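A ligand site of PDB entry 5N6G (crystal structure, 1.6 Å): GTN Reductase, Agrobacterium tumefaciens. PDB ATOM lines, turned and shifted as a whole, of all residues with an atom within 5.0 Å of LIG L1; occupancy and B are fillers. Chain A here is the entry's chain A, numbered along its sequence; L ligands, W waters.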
ATOM      1  N   ALA A  22      -3.518 -29.459  19.105  1.00  0.00           N
ATOM      2  CA  ALA A  22      -2.889 -28.501  20.006  1.00  0.00           C
ATOM      3  C   ALA A  22      -3.709 -27.195  20.084  1.00  0.00           C
ATOM      4  O   ALA A  22      -4.479 -26.875  19.166  1.00  0.00           O
ATOM      5  CB  ALA A  22      -1.480 -28.175  19.551  1.00  0.00           C
ATOM      6  N   PRO A  23      -3.548 -26.438  21.167  1.00  0.00           N
ATOM      7  CA  PRO A  23      -4.284 -25.176  21.311  1.00  0.00           C
ATOM      8  C   PRO A  23      -3.804 -24.158  20.277  1.00  0.00           C
ATOM      9  O   PRO A  23      -2.597 -23.972  20.082  1.00  0.00           O
ATOM     10  CB  PRO A  23      -3.940 -24.725  22.725  1.00  0.00           C
ATOM     11  CG  PRO A  23      -2.610 -25.397  23.041  1.00  0.00           C
ATOM     12  CD  PRO A  23      -2.690 -26.732  22.335  1.00  0.00           C
ATOM     13  N   LEU A  24      -4.755 -23.500  19.613  1.00  0.00           N
ATOM     14  CA  LEU A  24      -4.427 -22.571  18.541  1.00  0.00           C
ATOM     15  C   LEU A  24      -5.304 -21.328  18.607  1.00  0.00           C
ATOM     16  O   LEU A  24      -6.455 -21.351  18.156  1.00  0.00           O
ATOM     17  CB  LEU A  24      -4.588 -23.246  17.192  1.00  0.00           C
ATOM     18  CG  LEU A  24      -3.696 -24.461  16.936  1.00  0.00           C
ATOM     19  CD1 LEU A  24      -4.344 -25.358  15.880  1.00  0.00           C
ATOM     20  CD2 LEU A  24      -2.326 -23.985  16.505  1.00  0.00           C
ATOM     21  N   THR A  25      -4.735 -20.225  19.102  1.00  0.00           N
ATOM     22  CA  THR A  25      -5.384 -18.908  19.048  1.00  0.00           C
ATOM     23  C   THR A  25      -5.609 -18.480  17.603  1.00  0.00           C
ATOM     24  O   THR A  25      -4.686 -18.449  16.783  1.00  0.00           O
ATOM     25  CB  THR A  25      -4.482 -17.896  19.769  1.00  0.00           C
ATOM     26  OG1 THR A  25      -4.458 -18.224  21.162  1.00  0.00           O
ATOM     27  CG2 THR A  25      -5.006 -16.469  19.635  1.00  0.00           C
ATOM     28  N   ARG A  26      -6.867 -18.161  17.280  1.00  0.00           N
ATOM     29  CA  ARG A  26      -7.216 -17.738  15.933  1.00  0.00           C
ATOM     30  C   ARG A  26      -7.882 -16.366  15.867  1.00  0.00           C
ATOM     31  O   ARG A  26      -8.072 -15.866  14.765  1.00  0.00           O
ATOM     32  CB  ARG A  26      -8.159 -18.767  15.259  1.00  0.00           C
ATOM     33  CG  ARG A  26      -7.721 -20.261  15.417  1.00  0.00           C
ATOM     34  CD  ARG A  26      -6.365 -20.562  14.798  1.00  0.00           C
ATOM     35  NE  ARG A  26      -6.312 -20.137  13.400  1.00  0.00           N
ATOM     36  CZ  ARG A  26      -6.745 -20.861  12.369  1.00  0.00           C
ATOM     37  NH1 ARG A  26      -7.237 -22.080  12.552  1.00  0.00           N
ATOM     38  NH2 ARG A  26      -6.682 -20.360  11.149  1.00  0.00           N
ATOM     39  N   GLU A  54      -8.166 -23.297  21.605  1.00  0.00           N
ATOM     40  CA  GLU A  54      -7.432 -22.043  21.719  1.00  0.00           C
ATOM     41  C   GLU A  54      -7.433 -21.567  23.161  1.00  0.00           C
ATOM     42  O   GLU A  54      -8.378 -21.809  23.910  1.00  0.00           O
ATOM     43  CB  GLU A  54      -8.087 -20.980  20.834  1.00  0.00           C
ATOM     44  CG  GLU A  54      -9.506 -20.564  21.227  1.00  0.00           C
ATOM     45  CD  GLU A  54     -10.345 -20.103  20.037  1.00  0.00           C
ATOM     46  OE1 GLU A  54     -10.231 -18.925  19.613  1.00  0.00           O
ATOM     47  OE2 GLU A  54     -11.115 -20.933  19.507  1.00  0.00           O
ATOM     48  N   GLY A  55      -6.398 -20.843  23.549  1.00  0.00           N
ATOM     49  CA  GLY A  55      -6.393 -20.278  24.884  1.00  0.00           C
ATOM     50  C   GLY A  55      -7.655 -19.482  25.121  1.00  0.00           C
ATOM     51  O   GLY A  55      -8.085 -18.694  24.258  1.00  0.00           O
ATOM     52  N   GLN A  97      -8.461 -24.760  27.186  1.00  0.00           N
ATOM     53  CA  GLN A  97      -7.161 -24.267  27.638  1.00  0.00           C
ATOM     54  C   GLN A  97      -7.386 -22.969  28.398  1.00  0.00           C
ATOM     55  O   GLN A  97      -7.458 -21.904  27.801  1.00  0.00           O
ATOM     56  CB  GLN A  97      -6.170 -24.058  26.490  1.00  0.00           C
ATOM     57  CG  GLN A  97      -4.797 -23.751  27.078  1.00  0.00           C
ATOM     58  CD  GLN A  97      -3.730 -23.325  26.104  1.00  0.00           C
ATOM     59  OE1 GLN A  97      -3.900 -22.385  25.320  1.00  0.00           O
ATOM     60  NE2 GLN A  97      -2.593 -23.971  26.191  1.00  0.00           N
ATOM     61  N   HIS A 178      -3.094 -23.400  31.020  1.00  0.00           N
ATOM     62  CA  HIS A 178      -2.008 -22.811  30.231  1.00  0.00           C
ATOM     63  C   HIS A 178      -0.900 -22.347  31.157  1.00  0.00           C
ATOM     64  O   HIS A 178      -0.989 -21.266  31.753  1.00  0.00           O
ATOM     65  CB  HIS A 178      -2.523 -21.657  29.391  1.00  0.00           C
ATOM     66  CG  HIS A 178      -1.618 -21.298  28.260  1.00  0.00           C
ATOM     67  ND1 HIS A 178      -0.272 -21.568  28.249  1.00  0.00           N
ATOM     68  CD2 HIS A 178      -1.885 -20.703  27.065  1.00  0.00           C
ATOM     69  CE1 HIS A 178       0.258 -21.177  27.110  1.00  0.00           C
ATOM     70  NE2 HIS A 178      -0.697 -20.631  26.371  1.00  0.00           N
ATOM     71  N   ASN A 181       4.536 -20.807  27.436  1.00  0.00           N
ATOM     72  CA  ASN A 181       4.729 -19.716  26.460  1.00  0.00           C
ATOM     73  C   ASN A 181       4.736 -18.324  27.073  1.00  0.00           C
ATOM     74  O   ASN A 181       4.292 -17.358  26.462  1.00  0.00           O
ATOM     75  CB  ASN A 181       3.688 -19.810  25.353  1.00  0.00           C
ATOM     76  CG  ASN A 181       3.791 -21.112  24.613  1.00  0.00           C
ATOM     77  OD1 ASN A 181       4.870 -21.702  24.523  1.00  0.00           O
ATOM     78  ND2 ASN A 181       2.688 -21.578  24.081  1.00  0.00           N
ATOM     79  N   ARG A 230      -0.241 -27.523  30.448  1.00  0.00           N
ATOM     80  CA  ARG A 230       0.736 -27.378  29.376  1.00  0.00           C
ATOM     81  C   ARG A 230       1.983 -26.674  29.899  1.00  0.00           C
ATOM     82  O   ARG A 230       1.878 -25.612  30.527  1.00  0.00           O
ATOM     83  CB  ARG A 230       0.160 -26.602  28.192  1.00  0.00           C
ATOM     84  CG  ARG A 230       1.056 -26.694  26.971  1.00  0.00           C
ATOM     85  CD  ARG A 230       0.448 -26.100  25.735  1.00  0.00           C
ATOM     86  NE  ARG A 230       0.820 -26.881  24.563  1.00  0.00           N
ATOM     87  CZ  ARG A 230       1.008 -26.403  23.333  1.00  0.00           C
ATOM     88  NH1 ARG A 230       0.931 -25.114  23.090  1.00  0.00           N
ATOM     89  NH2 ARG A 230       1.280 -27.234  22.352  1.00  0.00           N
ATOM     90  N   VAL A 267       5.667 -28.791  25.403  1.00  0.00           N
ATOM     91  CA  VAL A 267       6.266 -28.195  24.206  1.00  0.00           C
ATOM     92  C   VAL A 267       7.755 -28.471  24.268  1.00  0.00           C
ATOM     93  O   VAL A 267       8.458 -28.013  25.172  1.00  0.00           O
ATOM     94  CB  VAL A 267       6.004 -26.681  24.141  1.00  0.00           C
ATOM     95  CG1 VAL A 267       6.674 -26.044  22.917  1.00  0.00           C
ATOM     96  CG2 VAL A 267       4.503 -26.373  24.149  1.00  0.00           C
ATOM     97  N   THR A 271       8.683 -22.816  20.985  1.00  0.00           N
ATOM     98  CA  THR A 271       7.350 -23.013  20.438  1.00  0.00           C
ATOM     99  C   THR A 271       7.321 -22.560  18.993  1.00  0.00           C
ATOM    100  O   THR A 271       7.541 -21.376  18.700  1.00  0.00           O
ATOM    101  CB  THR A 271       6.328 -22.229  21.250  1.00  0.00           C
ATOM    102  OG1 THR A 271       6.586 -22.406  22.651  1.00  0.00           O
ATOM    103  CG2 THR A 271       4.928 -22.750  20.927  1.00  0.00           C
ATOM    104  N   GLY A 272       7.043 -23.487  18.088  1.00  0.00           N
ATOM    105  CA  GLY A 272       7.034 -23.182  16.669  1.00  0.00           C
ATOM    106  C   GLY A 272       8.402 -23.028  16.048  1.00  0.00           C
ATOM    107  O   GLY A 272       8.492 -22.633  14.882  1.00  0.00           O
ATOM    108  N   ASN A 305       4.523 -32.119  21.981  1.00  0.00           N
ATOM    109  CA  ASN A 305       4.259 -31.191  20.907  1.00  0.00           C
ATOM    110  C   ASN A 305       5.555 -30.548  20.453  1.00  0.00           C
ATOM    111  O   ASN A 305       6.527 -30.462  21.213  1.00  0.00           O
ATOM    112  CB  ASN A 305       3.314 -30.081  21.359  1.00  0.00           C
ATOM    113  CG  ASN A 305       3.247 -28.953  20.385  1.00  0.00           C
ATOM    114  OD1 ASN A 305       3.897 -27.918  20.561  1.00  0.00           O
ATOM    115  ND2 ASN A 305       2.492 -29.135  19.319  1.00  0.00           N
ATOM    116  N   ASN A 306       5.533 -30.103  19.186  1.00  0.00           N
ATOM    117  CA  ASN A 306       6.375 -29.105  18.534  1.00  0.00           C
ATOM    118  C   ASN A 306       7.231 -29.765  17.446  1.00  0.00           C
ATOM    119  O   ASN A 306       8.191 -30.491  17.725  1.00  0.00           O
ATOM    120  CB  ASN A 306       7.246 -28.322  19.517  1.00  0.00           C
ATOM    121  CG  ASN A 306       7.912 -27.126  18.831  1.00  0.00           C
ATOM    122  OD1 ASN A 306       7.265 -26.364  18.110  1.00  0.00           O
ATOM    123  ND2 ASN A 306       9.230 -27.005  19.000  1.00  0.00           N
ATOM    124  N   GLY A 307       6.858 -29.527  16.197  1.00  0.00           N
ATOM    125  CA  GLY A 307       7.644 -30.001  15.075  1.00  0.00           C
ATOM    126  C   GLY A 307       7.473 -31.457  14.713  1.00  0.00           C
ATOM    127  O   GLY A 307       8.293 -31.983  13.949  1.00  0.00           O
ATOM    128  N   TYR A 308       6.456 -32.132  15.238  1.00  0.00           N
ATOM    129  CA  TYR A 308       6.238 -33.521  14.866  1.00  0.00           C
ATOM    130  C   TYR A 308       5.664 -33.610  13.458  1.00  0.00           C
ATOM    131  O   TYR A 308       4.994 -32.691  12.979  1.00  0.00           O
ATOM    132  CB  TYR A 308       5.281 -34.185  15.844  1.00  0.00           C
ATOM    133  CG  TYR A 308       5.945 -34.601  17.118  1.00  0.00           C
ATOM    134  CD1 TYR A 308       6.561 -35.834  17.221  1.00  0.00           C
ATOM    135  CD2 TYR A 308       5.981 -33.756  18.221  1.00  0.00           C
ATOM    136  CE1 TYR A 308       7.187 -36.237  18.375  1.00  0.00           C
ATOM    137  CE2 TYR A 308       6.628 -34.146  19.406  1.00  0.00           C
ATOM    138  CZ  TYR A 308       7.229 -35.398  19.463  1.00  0.00           C
ATOM    139  OH  TYR A 308       7.877 -35.832  20.589  1.00  0.00           O
ATOM    140  N   ALA A 326       0.481 -33.949  20.002  1.00  0.00           N
ATOM    141  CA  ALA A 326      -0.377 -32.828  19.661  1.00  0.00           C
ATOM    142  C   ALA A 326       0.219 -32.100  18.472  1.00  0.00           C
ATOM    143  O   ALA A 326       1.411 -31.768  18.467  1.00  0.00           O
ATOM    144  CB  ALA A 326      -0.539 -31.889  20.842  1.00  0.00           C
ATOM    145  N   PHE A 327      -0.604 -31.855  17.469  1.00  0.00           N
ATOM    146  CA  PHE A 327      -0.225 -31.156  16.258  1.00  0.00           C
ATOM    147  C   PHE A 327      -0.923 -29.819  16.228  1.00  0.00           C
ATOM    148  O   PHE A 327      -2.127 -29.754  16.466  1.00  0.00           O
ATOM    149  CB  PHE A 327      -0.635 -31.934  15.017  1.00  0.00           C
ATOM    150  CG  PHE A 327      -0.009 -33.311  14.896  1.00  0.00           C
ATOM    151  CD1 PHE A 327       1.158 -33.484  14.181  1.00  0.00           C
ATOM    152  CD2 PHE A 327      -0.616 -34.420  15.440  1.00  0.00           C
ATOM    153  CE1 PHE A 327       1.715 -34.741  14.014  1.00  0.00           C
ATOM    154  CE2 PHE A 327      -0.065 -35.687  15.307  1.00  0.00           C
ATOM    155  CZ  PHE A 327       1.094 -35.839  14.588  1.00  0.00           C
ATOM    156  N   GLY A 328      -0.172 -28.765  15.907  1.00  0.00           N
ATOM    157  CA  GLY A 328      -0.734 -27.430  15.800  1.00  0.00           C
ATOM    158  C   GLY A 328      -1.002 -27.028  14.358  1.00  0.00           C
ATOM    159  O   GLY A 328      -2.131 -27.133  13.865  1.00  0.00           O
ATOM    160  N   LYS A 329       0.042 -26.619  13.624  1.00  0.00           N
ATOM    161  CA  LYS A 329      -0.166 -26.098  12.282  1.00  0.00           C
ATOM    162  C   LYS A 329      -0.792 -27.131  11.361  1.00  0.00           C
ATOM    163  O   LYS A 329      -1.584 -26.783  10.482  1.00  0.00           O
ATOM    164  CB  LYS A 329       1.159 -25.587  11.713  1.00  0.00           C
ATOM    165  CG  LYS A 329       1.646 -24.323  12.434  1.00  0.00           C
ATOM    166  CD  LYS A 329       2.868 -23.739  11.761  1.00  0.00           C
ATOM    167  CE  LYS A 329       4.079 -24.631  11.944  1.00  0.00           C
ATOM    168  NZ  LYS A 329       4.419 -24.873  13.371  1.00  0.00           N
ATOM    169  N   ALA A 330      -0.488 -28.412  11.552  1.00  0.00           N
ATOM    170  CA  ALA A 330      -1.097 -29.410  10.680  1.00  0.00           C
ATOM    171  C   ALA A 330      -2.604 -29.503  10.893  1.00  0.00           C
ATOM    172  O   ALA A 330      -3.345 -29.799   9.944  1.00  0.00           O
ATOM    173  CB  ALA A 330      -0.453 -30.785  10.903  1.00  0.00           C
ATOM    174  N   ILE A 332      -4.482 -26.837  11.772  1.00  0.00           N
ATOM    175  CA  ILE A 332      -5.031 -25.669  11.078  1.00  0.00           C
ATOM    176  C   ILE A 332      -5.465 -26.053   9.681  1.00  0.00           C
ATOM    177  O   ILE A 332      -6.580 -25.737   9.237  1.00  0.00           O
ATOM    178  CB  ILE A 332      -4.008 -24.525  11.034  1.00  0.00           C
ATOM    179  CG1 ILE A 332      -3.796 -23.961  12.437  1.00  0.00           C
ATOM    180  CG2 ILE A 332      -4.455 -23.424  10.058  1.00  0.00           C
ATOM    181  CD1 ILE A 332      -2.705 -22.895  12.509  1.00  0.00           C
ATOM    182  N   PHE A 355      -3.722 -17.180   9.768  1.00  0.00           N
ATOM    183  CA  PHE A 355      -3.737 -17.789  11.092  1.00  0.00           C
ATOM    184  C   PHE A 355      -4.572 -16.958  12.066  1.00  0.00           C
ATOM    185  O   PHE A 355      -5.359 -17.508  12.844  1.00  0.00           O
ATOM    186  CB  PHE A 355      -2.316 -17.948  11.660  1.00  0.00           C
ATOM    187  CG  PHE A 355      -1.528 -19.127  11.101  1.00  0.00           C
ATOM    188  CD1 PHE A 355      -2.040 -19.957  10.130  1.00  0.00           C
ATOM    189  CD2 PHE A 355      -0.258 -19.379  11.579  1.00  0.00           C
ATOM    190  CE1 PHE A 355      -1.288 -21.028   9.624  1.00  0.00           C
ATOM    191  CE2 PHE A 355       0.492 -20.442  11.096  1.00  0.00           C
ATOM    192  CZ  PHE A 355      -0.025 -21.272  10.103  1.00  0.00           C
ATOM    193  N   TYR A 356      -4.411 -15.625  12.041  1.00  0.00           N
ATOM    194  CA  TYR A 356      -4.955 -14.763  13.088  1.00  0.00           C
ATOM    195  C   TYR A 356      -5.954 -13.783  12.507  1.00  0.00           C
ATOM    196  O   TYR A 356      -5.630 -13.030  11.591  1.00  0.00           O
ATOM    197  CB  TYR A 356      -3.849 -13.983  13.787  1.00  0.00           C
ATOM    198  CG  TYR A 356      -2.712 -14.861  14.244  1.00  0.00           C
ATOM    199  CD1 TYR A 356      -2.899 -15.742  15.291  1.00  0.00           C
ATOM    200  CD2 TYR A 356      -1.483 -14.818  13.624  1.00  0.00           C
ATOM    201  CE1 TYR A 356      -1.883 -16.561  15.714  1.00  0.00           C
ATOM    202  CE2 TYR A 356      -0.461 -15.631  14.040  1.00  0.00           C
ATOM    203  CZ  TYR A 356      -0.662 -16.495  15.076  1.00  0.00           C
ATOM    204  OH  TYR A 356       0.349 -17.319  15.504  1.00  0.00           O
HETATM  205  N1  LIG L   1      -0.047 -22.508  22.129  1.00  0.00           N
HETATM  206  C1  LIG L   1      -0.849 -22.451  23.252  1.00  0.00           C
HETATM  207  O1  LIG L   1      -0.522 -23.025  24.308  1.00  0.00           O
HETATM  208  N2  LIG L   1      -2.047 -21.784  23.196  1.00  0.00           N
HETATM  209  C2  LIG L   1      -2.542 -21.086  22.109  1.00  0.00           C
HETATM  210  O2  LIG L   1      -3.654 -20.557  22.145  1.00  0.00           O
HETATM  211  C3  LIG L   1      -1.683 -21.124  20.939  1.00  0.00           C
HETATM  212  N3  LIG L   1      -2.094 -20.514  19.859  1.00  0.00           N
HETATM  213  C4  LIG L   1      -1.337 -20.686  18.701  1.00  0.00           C
HETATM  214  C5  LIG L   1      -1.824 -20.154  17.514  1.00  0.00           C
HETATM  215  C6  LIG L   1      -1.169 -20.396  16.314  1.00  0.00           C
HETATM  216  C7  LIG L   1      -1.751 -19.814  15.041  1.00  0.00           C
HETATM  217  C8  LIG L   1      -0.010 -21.167  16.288  1.00  0.00           C
HETATM  218  C9  LIG L   1       0.681 -21.510  14.993  1.00  0.00           C
HETATM  219  C10 LIG L   1       0.494 -21.697  17.475  1.00  0.00           C
HETATM  220  C11 LIG L   1      -0.177 -21.470  18.680  1.00  0.00           C
HETATM  221  N4  LIG L   1       0.242 -22.078  19.882  1.00  0.00           N
HETATM  222  C12 LIG L   1      -0.475 -21.897  21.034  1.00  0.00           C
HETATM  223  C13 LIG L   1       1.340 -23.046  19.828  1.00  0.00           C
HETATM  224  C14 LIG L   1       0.855 -24.391  19.295  1.00  0.00           C
HETATM  225  O3  LIG L   1      -0.071 -24.992  20.213  1.00  0.00           O
HETATM  226  C15 LIG L   1       1.991 -25.375  19.031  1.00  0.00           C
HETATM  227  O4  LIG L   1       2.761 -25.548  20.218  1.00  0.00           O
HETATM  228  C16 LIG L   1       2.935 -24.941  17.906  1.00  0.00           C
HETATM  229  O5  LIG L   1       2.174 -24.627  16.729  1.00  0.00           O
HETATM  230  C17 LIG L   1       3.997 -25.984  17.603  1.00  0.00           C
HETATM  231  O6  LIG L   1       3.382 -27.214  17.144  1.00  0.00           O
HETATM  232  P1  LIG L   1       3.351 -27.687  15.594  1.00  0.00           P
HETATM  233  O7  LIG L   1       4.805 -27.871  15.204  1.00  0.00           O
HETATM  234  O8  LIG L   1       2.714 -26.547  14.830  1.00  0.00           O
HETATM  235  O9  LIG L   1       2.556 -28.949  15.615  1.00  0.00           O
HETATM  236  C1  LG2 L   2      -0.052 -17.190  18.976  1.00  0.00           C
HETATM  237  C2  LG2 L   2      -0.676 -15.964  18.958  1.00  0.00           C
HETATM  238  C3  LG2 L   2      -1.261 -15.477  20.107  1.00  0.00           C
HETATM  239  C4  LG2 L   2      -1.233 -16.225  21.272  1.00  0.00           C
HETATM  240  C5  LG2 L   2       0.539 -19.046  22.962  1.00  0.00           C
HETATM  241  C6  LG2 L   2      -1.817 -18.404  23.214  1.00  0.00           C
HETATM  242  O1  LG2 L   2       0.477 -19.859  23.857  1.00  0.00           O
HETATM  243  C7  LG2 L   2      -0.694 -18.322  22.520  1.00  0.00           C
HETATM  244  C8  LG2 L   2      -0.619 -17.474  21.294  1.00  0.00           C
HETATM  245  C9  LG2 L   2      -0.013 -17.940  20.135  1.00  0.00           C
HETATM  246  O2  LG2 L   2       1.665 -18.747  22.361  1.00  0.00           O
HETATM  247  O   HOH W   1       3.870 -31.049  16.974  1.00  0.00           O
HETATM  248  O   HOH W   2       1.610 -29.708  13.086  1.00  0.00           O
HETATM  249  O   HOH W   3       4.106 -22.643  15.175  1.00  0.00           O
HETATM  250  O   HOH W   4       5.136 -29.746  13.131  1.00  0.00           O
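The side-chain amino group (NZ) of Lys 329 is in salt-bridge range of an oxygen (O8) of LIG L1 (2.8 Å).
The side-chain hydroxyl (OG1) of Thr 25 sits at hydrogen-bond distance from an oxygen (O2) of LIG L1, 2.7 Å away.
N of Gly 55 is in hydrogen-bond range of O2 of LIG L1 (3.1 Å).
An oxygen (O1) of LIG L1 sits at hydrogen-bond distance from a ring nitrogen (NE2) of His 178 (3.2 Å).
An oxygen (O1) of LG2 L2 sits at hydrogen-bond distance from a ring nitrogen (NE2) of His 178 (2.9 Å).
O7 of LIG L1 sits at hydrogen-bond distance from N of Gly 307 (2.8 Å).
The backbone NH of Lys 329 lies within hydrogen-bond range of an oxygen (O8) of LIG L1 (2.9 Å).
An oxygen (O1) of LG2 L2 sits at hydrogen-bond distance from the side-chain amide nitrogen of Asn 181 (2.8 Å).
OE1 of Gln 97 sits at hydrogen-bond distance from N2 of LIG L1, at 2.9 Å.
An oxygen (O3) of LIG L1 sits at hydrogen-bond distance from the backbone carbonyl oxygen (O) of Pro 23 (2.7 Å).
An oxygen (O4) of LIG L1 sits at hydrogen-bond distance from the side-chain amide oxygen (OD1) of Asn 305 (2.7 Å).
An oxygen (O9) of LIG L1 is in hydrogen-bond range of the backbone NH (N) of Gly 328, 2.7 Å away.
The guanidinium group (NH1) of Arg 230 is in hydrogen-bond range of an oxygen (O1) of LIG L1 (2.8 Å).
The side-chain amide nitrogen (ND2) of Asn 181 is in hydrogen-bond range of a nitrogen (N1) of LIG L1 (3.5 Å).
The backbone NH of Thr 25 lies within hydrogen-bond range of a nitrogen (N3) of LIG L1.
A nitrogen (N2) of LIG L1 sits close to an oxygen (O1) of LG2 L2 (3.2 Å).
The side-chain amide oxygen of Gln 97 sits close to the backbone NH of Gly 55, at 3.4 Å.
The side-chain amide oxygen (OD1) of Asn 181 is in hydrogen-bond range of the side-chain hydroxyl (OG1) of Thr 271 (2.6 Å).
The backbone NH (N) of Ala 22 lies within hydrogen-bond range of the backbone carbonyl oxygen (O) of Phe 327, at 3.0 Å.
The backbone carbonyl oxygen of Phe 355 sits at hydrogen-bond distance from the guanidinium group of Arg 26 (2.9 Å).
NH2 of Arg 230 sits at hydrogen-bond distance from OD1 of Asn 305, at 3.2 Å.
The side-chain amide oxygen of Asn 306 sits at hydrogen-bond distance from the backbone NH of Gly 272 (2.9 Å).
O of Ala 326 is in hydrogen-bond range of ND2 of Asn 305, at 3.0 Å.
Residues that only touch LIG L1: Ala 22, Leu 24, Thr 271, Gly 272, Asn 306, Phe 327, Phe 355 and Tyr 356.
Hydrophobic or aromatic side chains that line LIG L1: Ala 22, Pro 23, Leu 24, His 178, Phe 355 and Tyr 356.
Water W2 lies within hydrogen-bond range of an oxygen (O9) of LIG L1 (2.8 Å), the backbone NH of Ala 330 (2.9 Å) and the backbone NH of Gly 328 (3.5 Å).
Water W4 bridges O7 of LIG L1 (2.8 Å) and O of Tyr 308 (3.0 Å).
Water W3 lies within hydrogen-bond range of NZ of Lys 329 (2.9 Å) and O5 of LIG L1 (3.2 Å).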
